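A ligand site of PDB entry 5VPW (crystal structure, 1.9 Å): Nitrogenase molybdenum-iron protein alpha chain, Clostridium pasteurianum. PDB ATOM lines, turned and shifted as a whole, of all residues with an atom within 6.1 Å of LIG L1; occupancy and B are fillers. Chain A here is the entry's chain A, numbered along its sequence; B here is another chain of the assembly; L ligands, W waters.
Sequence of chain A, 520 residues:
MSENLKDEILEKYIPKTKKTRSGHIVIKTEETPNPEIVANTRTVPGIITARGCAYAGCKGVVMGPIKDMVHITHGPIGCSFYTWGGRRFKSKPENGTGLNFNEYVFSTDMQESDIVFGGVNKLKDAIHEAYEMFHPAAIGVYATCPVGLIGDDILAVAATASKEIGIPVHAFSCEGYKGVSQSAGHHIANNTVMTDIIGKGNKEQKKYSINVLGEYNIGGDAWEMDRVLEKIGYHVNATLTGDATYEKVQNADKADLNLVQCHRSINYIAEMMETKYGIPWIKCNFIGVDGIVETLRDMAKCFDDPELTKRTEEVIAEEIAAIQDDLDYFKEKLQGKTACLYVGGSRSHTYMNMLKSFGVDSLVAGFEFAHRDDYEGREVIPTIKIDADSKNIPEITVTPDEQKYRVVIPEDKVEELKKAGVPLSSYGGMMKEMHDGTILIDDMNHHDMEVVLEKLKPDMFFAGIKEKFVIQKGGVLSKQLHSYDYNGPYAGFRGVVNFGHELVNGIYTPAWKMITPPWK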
ATOM      1  N   ALA A  50      17.633  15.238 -14.685  1.00  0.00           N
ATOM      2  CA  ALA A  50      18.814  15.165 -13.823  1.00  0.00           C
ATOM      3  C   ALA A  50      18.938  16.407 -13.005  1.00  0.00           C
ATOM      4  O   ALA A  50      19.892  16.504 -12.249  1.00  0.00           O
ATOM      5  CB  ALA A  50      20.078  14.972 -14.646  1.00  0.00           C
ATOM      6  N   GLY A  52      18.697  19.360 -10.173  1.00  0.00           N
ATOM      7  CA  GLY A  52      18.580  19.535  -8.743  1.00  0.00           C
ATOM      8  C   GLY A  52      17.844  20.817  -8.425  1.00  0.00           C
ATOM      9  O   GLY A  52      17.145  21.365  -9.287  1.00  0.00           O
ATOM     10  N   ALA A  56      20.686  23.163  -3.597  1.00  0.00           N
ATOM     11  CA  ALA A  56      21.928  22.598  -4.182  1.00  0.00           C
ATOM     12  C   ALA A  56      22.759  23.670  -4.874  1.00  0.00           C
ATOM     13  O   ALA A  56      23.989  23.764  -4.694  1.00  0.00           O
ATOM     14  CB  ALA A  56      21.639  21.482  -5.139  1.00  0.00           C
ATOM     15  N   GLY A  57      22.114  24.516  -5.631  1.00  0.00           N
ATOM     16  CA  GLY A  57      22.828  25.597  -6.316  1.00  0.00           C
ATOM     17  C   GLY A  57      23.478  26.596  -5.364  1.00  0.00           C
ATOM     18  O   GLY A  57      24.576  27.108  -5.630  1.00  0.00           O
ATOM     19  N   VAL A  61      26.788  24.342  -4.136  1.00  0.00           N
ATOM     20  CA  VAL A  61      27.636  24.758  -5.262  1.00  0.00           C
ATOM     21  C   VAL A  61      28.433  26.026  -5.012  1.00  0.00           C
ATOM     22  O   VAL A  61      29.671  25.979  -4.912  1.00  0.00           O
ATOM     23  CB  VAL A  61      26.784  24.871  -6.566  1.00  0.00           C
ATOM     24  CG1 VAL A  61      27.629  25.375  -7.716  1.00  0.00           C
ATOM     25  CG2 VAL A  61      26.207  23.504  -6.915  1.00  0.00           C
ATOM     26  N   GLY A  86      30.055  14.806  -1.709  1.00  0.00           N
ATOM     27  CA  GLY A  86      29.753  14.355  -3.062  1.00  0.00           C
ATOM     28  C   GLY A  86      30.286  15.264  -4.151  1.00  0.00           C
ATOM     29  O   GLY A  86      30.605  14.782  -5.225  1.00  0.00           O
ATOM     30  N   ARG A  87      30.341  16.570  -3.871  1.00  0.00           N
ATOM     31  CA  ARG A  87      30.892  17.516  -4.824  1.00  0.00           C
ATOM     32  C   ARG A  87      32.345  17.793  -4.373  1.00  0.00           C
ATOM     33  O   ARG A  87      32.554  18.200  -3.241  1.00  0.00           O
ATOM     34  CB  ARG A  87      30.086  18.804  -4.858  1.00  0.00           C
ATOM     35  CG  ARG A  87      30.631  19.792  -5.923  1.00  0.00           C
ATOM     36  CD  ARG A  87      29.579  20.826  -6.308  1.00  0.00           C
ATOM     37  NE  ARG A  87      30.100  21.958  -7.109  1.00  0.00           N
ATOM     38  CZ  ARG A  87      30.559  23.089  -6.594  1.00  0.00           C
ATOM     39  NH1 ARG A  87      30.951  24.073  -7.417  1.00  0.00           N
ATOM     40  NH2 ARG A  87      30.553  23.298  -5.283  1.00  0.00           N
ATOM     41  N   ARG A  88      33.300  17.612  -5.290  1.00  0.00           N
ATOM     42  CA  ARG A  88      34.720  17.432  -4.941  1.00  0.00           C
ATOM     43  C   ARG A  88      35.548  18.741  -4.963  1.00  0.00           C
ATOM     44  O   ARG A  88      36.678  18.799  -5.497  1.00  0.00           O
ATOM     45  CB  ARG A  88      35.336  16.377  -5.859  1.00  0.00           C
ATOM     46  CG  ARG A  88      34.722  15.004  -5.681  1.00  0.00           C
ATOM     47  CD  ARG A  88      35.339  13.963  -6.591  1.00  0.00           C
ATOM     48  NE  ARG A  88      36.794  13.859  -6.347  1.00  0.00           N
ATOM     49  CZ  ARG A  88      37.739  14.273  -7.177  1.00  0.00           C
ATOM     50  NH1 ARG A  88      39.020  14.190  -6.809  1.00  0.00           N
ATOM     51  NH2 ARG A  88      37.424  14.745  -8.369  1.00  0.00           N
ATOM     52  N   GLN A 182      19.147  24.255 -10.223  1.00  0.00           N
ATOM     53  CA  GLN A 182      20.263  24.814  -9.428  1.00  0.00           C
ATOM     54  C   GLN A 182      20.496  26.285  -9.660  1.00  0.00           C
ATOM     55  O   GLN A 182      21.021  26.972  -8.782  1.00  0.00           O
ATOM     56  CB  GLN A 182      21.594  24.080  -9.742  1.00  0.00           C
ATOM     57  CG  GLN A 182      21.657  22.623  -9.345  1.00  0.00           C
ATOM     58  CD  GLN A 182      21.218  21.665 -10.452  1.00  0.00           C
ATOM     59  OE1 GLN A 182      20.190  21.840 -11.093  1.00  0.00           O
ATOM     60  NE2 GLN A 182      22.002  20.629 -10.655  1.00  0.00           N
ATOM     61  N   GLU A 368      21.364  20.365 -18.340  1.00  0.00           N
ATOM     62  CA  GLU A 368      20.334  20.348 -17.299  1.00  0.00           C
ATOM     63  C   GLU A 368      19.568  21.653 -17.287  1.00  0.00           C
ATOM     64  O   GLU A 368      18.316  21.656 -17.323  1.00  0.00           O
ATOM     65  CB  GLU A 368      20.931  20.116 -15.924  1.00  0.00           C
ATOM     66  CG  GLU A 368      21.530  18.738 -15.747  1.00  0.00           C
ATOM     67  CD  GLU A 368      21.973  18.396 -14.334  1.00  0.00           C
ATOM     68  OE1 GLU A 368      22.750  17.409 -14.249  1.00  0.00           O
ATOM     69  OE2 GLU A 368      21.530  19.035 -13.344  1.00  0.00           O
ATOM     70  N   PHE A 369      20.281  22.761 -17.222  1.00  0.00           N
ATOM     71  CA  PHE A 369      19.644  24.020 -16.797  1.00  0.00           C
ATOM     72  C   PHE A 369      20.231  25.316 -17.314  1.00  0.00           C
ATOM     73  O   PHE A 369      19.963  26.381 -16.708  1.00  0.00           O
ATOM     74  CB  PHE A 369      19.632  24.093 -15.273  1.00  0.00           C
ATOM     75  CG  PHE A 369      20.984  23.993 -14.658  1.00  0.00           C
ATOM     76  CD1 PHE A 369      21.883  25.050 -14.716  1.00  0.00           C
ATOM     77  CD2 PHE A 369      21.363  22.820 -14.066  1.00  0.00           C
ATOM     78  CE1 PHE A 369      23.142  24.905 -14.163  1.00  0.00           C
ATOM     79  CE2 PHE A 369      22.622  22.674 -13.513  1.00  0.00           C
ATOM     80  CZ  PHE A 369      23.491  23.722 -13.551  1.00  0.00           C
ATOM     81  N   ALA A 463      28.679  12.167 -18.919  1.00  0.00           N
ATOM     82  CA  ALA A 463      27.538  12.674 -18.155  1.00  0.00           C
ATOM     83  C   ALA A 463      27.812  12.809 -16.668  1.00  0.00           C
ATOM     84  O   ALA A 463      28.906  13.260 -16.263  1.00  0.00           O
ATOM     85  CB  ALA A 463      26.286  11.821 -18.452  1.00  0.00           C
ATOM     86  N   GLY A 464      26.824  12.494 -15.842  1.00  0.00           N
ATOM     87  CA  GLY A 464      26.998  12.499 -14.400  1.00  0.00           C
ATOM     88  C   GLY A 464      26.811  11.116 -13.782  1.00  0.00           C
ATOM     89  O   GLY A 464      26.765  10.106 -14.509  1.00  0.00           O
ATOM     90  N   ILE A 465      26.667  11.076 -12.462  1.00  0.00           N
ATOM     91  CA  ILE A 465      26.592   9.805 -11.714  1.00  0.00           C
ATOM     92  C   ILE A 465      25.275   9.057 -11.934  1.00  0.00           C
ATOM     93  O   ILE A 465      25.261   7.833 -11.951  1.00  0.00           O
ATOM     94  CB  ILE A 465      26.908  10.013 -10.206  1.00  0.00           C
ATOM     95  CG1 ILE A 465      27.189   8.698  -9.471  1.00  0.00           C
ATOM     96  CG2 ILE A 465      25.809  10.810  -9.513  1.00  0.00           C
ATOM     97  CD1 ILE A 465      28.294   7.845 -10.061  1.00  0.00           C
ATOM     98  N   LYS A 466      24.180   9.795 -12.151  1.00  0.00           N
ATOM     99  CA  LYS A 466      22.858   9.144 -12.374  1.00  0.00           C
ATOM    100  C   LYS A 466      22.776   8.430 -13.712  1.00  0.00           C
ATOM    101  O   LYS A 466      22.079   7.438 -13.855  1.00  0.00           O
ATOM    102  CB  LYS A 466      21.734  10.166 -12.230  1.00  0.00           C
ATOM    103  CG  LYS A 466      21.646  10.752 -10.812  1.00  0.00           C
ATOM    104  CD  LYS A 466      20.425  11.606 -10.506  1.00  0.00           C
ATOM    105  CE  LYS A 466      20.216  12.767 -11.473  1.00  0.00           C
ATOM    106  NZ  LYS A 466      21.225  13.824 -11.349  1.00  0.00           N
ATOM    107  N   GLU A 467      23.481   8.960 -14.691  1.00  0.00           N
ATOM    108  CA  GLU A 467      23.461   8.429 -16.047  1.00  0.00           C
ATOM    109  C   GLU A 467      24.602   7.472 -16.343  1.00  0.00           C
ATOM    110  O   GLU A 467      24.483   6.633 -17.258  1.00  0.00           O
ATOM    111  CB  GLU A 467      23.544   9.587 -17.054  1.00  0.00           C
ATOM    112  CG  GLU A 467      22.479  10.663 -16.861  1.00  0.00           C
ATOM    113  CD  GLU A 467      22.848  11.704 -15.809  1.00  0.00           C
ATOM    114  OE1 GLU A 467      24.063  11.872 -15.437  1.00  0.00           O
ATOM    115  OE2 GLU A 467      21.899  12.348 -15.334  1.00  0.00           O
ATOM    116  N   GLN A 480      32.544  10.706 -16.186  1.00  0.00           N
ATOM    117  CA  GLN A 480      31.842  11.744 -15.478  1.00  0.00           C
ATOM    118  C   GLN A 480      32.477  13.122 -15.655  1.00  0.00           C
ATOM    119  O   GLN A 480      33.646  13.304 -15.414  1.00  0.00           O
ATOM    120  CB  GLN A 480      31.782  11.433 -13.974  1.00  0.00           C
ATOM    121  CG  GLN A 480      31.007  10.190 -13.629  1.00  0.00           C
ATOM    122  CD  GLN A 480      30.889   9.985 -12.129  1.00  0.00           C
ATOM    123  OE1 GLN A 480      30.216  10.750 -11.406  1.00  0.00           O
ATOM    124  NE2 GLN A 480      31.578   8.953 -11.638  1.00  0.00           N
ATOM    125  N   HIS A 482      31.250  15.849 -13.934  1.00  0.00           N
ATOM    126  CA  HIS A 482      31.141  16.607 -12.732  1.00  0.00           C
ATOM    127  C   HIS A 482      32.221  16.174 -11.722  1.00  0.00           C
ATOM    128  O   HIS A 482      33.082  16.981 -11.340  1.00  0.00           O
ATOM    129  CB  HIS A 482      29.782  16.523 -12.023  1.00  0.00           C
ATOM    130  CG  HIS A 482      28.575  16.701 -12.880  1.00  0.00           C
ATOM    131  ND1 HIS A 482      27.639  17.699 -12.657  1.00  0.00           N
ATOM    132  CD2 HIS A 482      28.093  15.973 -13.914  1.00  0.00           C
ATOM    133  CE1 HIS A 482      26.636  17.553 -13.507  1.00  0.00           C
ATOM    134  NE2 HIS A 482      26.890  16.528 -14.278  1.00  0.00           N
ATOM    135  N   SER A 483      32.162  14.914 -11.284  1.00  0.00           N
ATOM    136  CA  SER A 483      33.127  14.373 -10.311  1.00  0.00           C
ATOM    137  C   SER A 483      34.489  13.993 -10.888  1.00  0.00           C
ATOM    138  O   SER A 483      35.410  13.658 -10.117  1.00  0.00           O
ATOM    139  CB  SER A 483      32.534  13.104  -9.670  1.00  0.00           C
ATOM    140  OG  SER A 483      32.438  12.045 -10.625  1.00  0.00           O
ATOM    141  N   SER B  50      16.846  13.735  -7.301  1.00  0.00           N
ATOM    142  CA  SER B  50      18.180  13.656  -7.827  1.00  0.00           C
ATOM    143  C   SER B  50      19.169  13.192  -6.759  1.00  0.00           C
ATOM    144  O   SER B  50      20.024  12.346  -7.025  1.00  0.00           O
ATOM    145  CB  SER B  50      18.621  15.009  -8.393  1.00  0.00           C
ATOM    146  OG  SER B  50      20.004  14.964  -8.699  1.00  0.00           O
ATOM    147  N   TYR B  51      19.030  13.712  -5.529  1.00  0.00           N
ATOM    148  CA  TYR B  51      19.979  13.338  -4.461  1.00  0.00           C
ATOM    149  C   TYR B  51      19.798  11.863  -4.048  1.00  0.00           C
ATOM    150  O   TYR B  51      20.764  11.134  -3.759  1.00  0.00           O
ATOM    151  CB  TYR B  51      19.811  14.241  -3.248  1.00  0.00           C
ATOM    152  CG  TYR B  51      20.514  15.583  -3.226  1.00  0.00           C
ATOM    153  CD1 TYR B  51      21.687  15.843  -3.941  1.00  0.00           C
ATOM    154  CD2 TYR B  51      20.051  16.571  -2.398  1.00  0.00           C
ATOM    155  CE1 TYR B  51      22.342  17.068  -3.798  1.00  0.00           C
ATOM    156  CE2 TYR B  51      20.668  17.785  -2.289  1.00  0.00           C
ATOM    157  CZ  TYR B  51      21.806  18.037  -3.002  1.00  0.00           C
ATOM    158  OH  TYR B  51      22.360  19.253  -2.824  1.00  0.00           O
ATOM    159  N   THR B  54      21.024   9.537  -6.579  1.00  0.00           N
ATOM    160  CA  THR B  54      22.476   9.646  -6.598  1.00  0.00           C
ATOM    161  C   THR B  54      23.158   8.751  -5.574  1.00  0.00           C
ATOM    162  O   THR B  54      24.130   8.045  -5.859  1.00  0.00           O
ATOM    163  CB  THR B  54      22.888  11.112  -6.456  1.00  0.00           C
ATOM    164  OG1 THR B  54      22.597  11.825  -7.691  1.00  0.00           O
ATOM    165  CG2 THR B  54      24.359  11.216  -6.144  1.00  0.00           C
ATOM    166  N   ARG B  58      25.899   5.761  -6.167  1.00  0.00           N
ATOM    167  CA  ARG B  58      27.226   5.758  -5.520  1.00  0.00           C
ATOM    168  C   ARG B  58      27.487   4.493  -4.676  1.00  0.00           C
ATOM    169  O   ARG B  58      28.621   4.012  -4.608  1.00  0.00           O
ATOM    170  CB  ARG B  58      27.416   6.990  -4.681  1.00  0.00           C
ATOM    171  CG  ARG B  58      27.507   8.281  -5.497  1.00  0.00           C
ATOM    172  CD  ARG B  58      27.478   9.522  -4.621  1.00  0.00           C
ATOM    173  NE  ARG B  58      27.757  10.699  -5.419  1.00  0.00           N
ATOM    174  CZ  ARG B  58      27.433  11.948  -5.091  1.00  0.00           C
ATOM    175  NH1 ARG B  58      26.832  12.237  -3.921  1.00  0.00           N
ATOM    176  NH2 ARG B  58      27.737  12.922  -5.968  1.00  0.00           N
HETATM  177  C1  LIG L   1      24.574  19.190  -7.967  1.00  0.00           C
HETATM  178  C2  LIG L   1      25.996  18.734  -7.729  1.00  0.00           C
HETATM  179  C3  LIG L   1      26.550  17.985  -8.948  1.00  0.00           C
HETATM  180  C4  LIG L   1      26.054  16.543  -9.091  1.00  0.00           C
HETATM  181  C5  LIG L   1      26.948  15.736 -10.074  1.00  0.00           C
HETATM  182  C6  LIG L   1      26.343  14.477 -10.712  1.00  0.00           C
HETATM  183  C7  LIG L   1      28.069  17.896  -8.813  1.00  0.00           C
HETATM  184  O1  LIG L   1      23.807  19.270  -6.974  1.00  0.00           O
HETATM  185  O2  LIG L   1      24.233  19.515  -9.125  1.00  0.00           O
HETATM  186  O3  LIG L   1      27.152  13.532 -10.947  1.00  0.00           O
HETATM  187  O4  LIG L   1      25.120  14.410 -10.993  1.00  0.00           O
HETATM  188  O5  LIG L   1      28.530  17.344  -7.824  1.00  0.00           O
HETATM  189  O6  LIG L   1      28.815  18.269  -9.738  1.00  0.00           O
HETATM  190  O7  LIG L   1      26.214  18.747 -10.117  1.00  0.00           O
HETATM  191 FE1  LG2 L   2      28.856  26.228 -13.355  1.00  0.00          FE
HETATM  192 MO1  LG2 L   2      27.766  19.635 -11.244  1.00  0.00          MO
HETATM  193 FE2  LG2 L   2      27.195  24.572 -12.020  1.00  0.00          FE
HETATM  194 FE3  LG2 L   2      29.837  24.222 -11.867  1.00  0.00          FE
HETATM  195 FE4  LG2 L   2      28.504  23.704 -14.132  1.00  0.00          FE
HETATM  196 FE5  LG2 L   2      28.069  21.245 -13.332  1.00  0.00          FE
HETATM  197 FE6  LG2 L   2      26.850  22.156 -11.221  1.00  0.00          FE
HETATM  198 FE7  LG2 L   2      29.409  21.754 -11.121  1.00  0.00          FE
HETATM  199  C1  LG2 L   2      28.330  22.960 -12.349  1.00  0.00           C
HETATM  200  S1  LG2 L   2      26.925  25.329 -14.169  1.00  0.00           S
HETATM  201  S2  LG2 L   2      26.045  20.594 -12.548  1.00  0.00           S
HETATM  202  S3  LG2 L   2      28.667  25.997 -11.089  1.00  0.00           S
HETATM  203  S4  LG2 L   2      25.537  23.836 -10.732  1.00  0.00           S
HETATM  204  S5  LG2 L   2      28.277  21.944 -15.435  1.00  0.00           S
HETATM  205  S6  LG2 L   2      27.943  21.227  -9.479  1.00  0.00           S
HETATM  206  S7  LG2 L   2      30.532  24.748 -13.914  1.00  0.00           S
HETATM  207  S8  LG2 L   2      29.764  20.011 -12.500  1.00  0.00           S
HETATM  208  S9  LG2 L   2      31.169  22.902 -10.494  1.00  0.00           S
HETATM  209  O   HOH W   1      23.222  16.480 -11.741  1.00  0.00           O
HETATM  210  O   HOH W   2      23.108  14.049  -9.091  1.00  0.00           O
HETATM  211  O   HOH W   3      21.419  18.383  -7.357  1.00  0.00           O
HETATM  212  O   HOH W   4      31.447  19.115  -9.296  1.00  0.00           O
HETATM  213  O   HOH W   5      24.586  19.639  -4.215  1.00  0.00           O
HETATM  214  O   HOH W   6      23.806  12.736 -12.576  1.00  0.00           O
HETATM  215  O   HOH W   7      30.164  15.190  -7.922  1.00  0.00           O
HETATM  216  O   HOH W   8      27.226  15.953  -5.626  1.00  0.00           O
HETATM  217  O   HOH W   9      29.686  13.341 -12.088  1.00  0.00           O
HETATM  218  O   HOH W  10      28.784  12.963  -8.762  1.00  0.00           O
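The side-chain amide nitrogen (NE2) of Gln 182 sits at hydrogen-bond distance from an oxygen (O2) of LIG L1, at 2.9 Å. O3 of LIG L1 sits at hydrogen-bond distance from N of Ile 465 (2.9 Å). O4 of LIG L1 is in salt-bridge range of NZ of Lys 466 (3.95 Å). ND1 of His 482 binds MO1 of LG2 L2, at 2.4 Å. A sulfur (S6) of LG2 L2 lies close to the guanidinium group (NE) of Arg 87, at 3.3 Å.
MO1 of LG2 L2 is bound by O7 of LIG L1.
The side-chain carboxylate (OE2) of Glu 368 lies within hydrogen-bond range of the side-chain amide nitrogen (NE2) of Gln 182 (3.2 Å). The side-chain amide oxygen (OE1) of Gln 182 is in hydrogen-bond range of the backbone NH (N) of Gly 52. O of Ala 56 is in hydrogen-bond range of N of Val 61, 2.9 Å away. The backbone NH (N) of Gly 464 lies within hydrogen-bond range of the side-chain carboxylate (OE1) of Glu 467. The guanidinium group of Arg 87 sits at hydrogen-bond distance from the backbone carbonyl oxygen of Val 61 (2.8 Å). The side-chain amino group of Lys 466 sits at hydrogen-bond distance from the side-chain hydroxyl of Ser 50 of chain B, 3.1 Å away. The side-chain amino group of Lys 466 sits at hydrogen-bond distance from the backbone carbonyl oxygen of Ala 50 of chain A (3.1 Å).
ND1 of His 482 sits close to O7 of LIG L1 (3.1 Å). Ala 56 touches LIG L1. Arg 87 touches LIG L1 (CB to O5, 3.7 Å). Gly 464 touches LIG L1. Hydrophobic or aromatic side chains within 4 Å of LIG L1: Ala 56, Ile 465 and His 482. Seven residues have an atom within 4 Å of LIG L1: Ala 56, Arg 87, Gln 182, Gly 464, Ile 465, Lys 466 and His 482. Along chain A the residues within 4 Å of LIG L1 span positions 56 to 482.
Water W6 lies within hydrogen-bond range of an oxygen (O4) of LIG L1, the backbone NH of Lys 466, the side-chain carboxylate of Glu 467 and the backbone NH of Ile 465. Water W10 lies within hydrogen-bond range of O3 of LIG L1 (2.8 Å) and NH2 of Arg 58 of chain B (3.0 Å). Water W2 lies within hydrogen-bond range of OG1 of Thr 54 of chain B (2.7 Å), O4 of LIG L1 (2.8 Å), NZ of Lys 466 (2.9 Å) and OG of Ser 50 of chain B (3.3 Å). Water W4 lies within hydrogen-bond range of the backbone carbonyl oxygen (O) of His 482 (3.4 Å) and a sulfur (S8) of LG2 L2 (3.7 Å). Water W1 lies within hydrogen-bond range of the side-chain carboxylate (OE1) of Glu 368 (2.7 Å), an oxygen (O4) of LIG L1 (2.9 Å), the side-chain amino group (NZ) of Lys 466 (3.3 Å) and the backbone carbonyl oxygen (O) of Ala 50 of chain A (3.4 Å). Water W8 lies within hydrogen-bond range of an oxygen (O5) of LIG L1 (2.9 Å) and the guanidinium group (NH2) of Arg 58 of chain B (3.1 Å).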
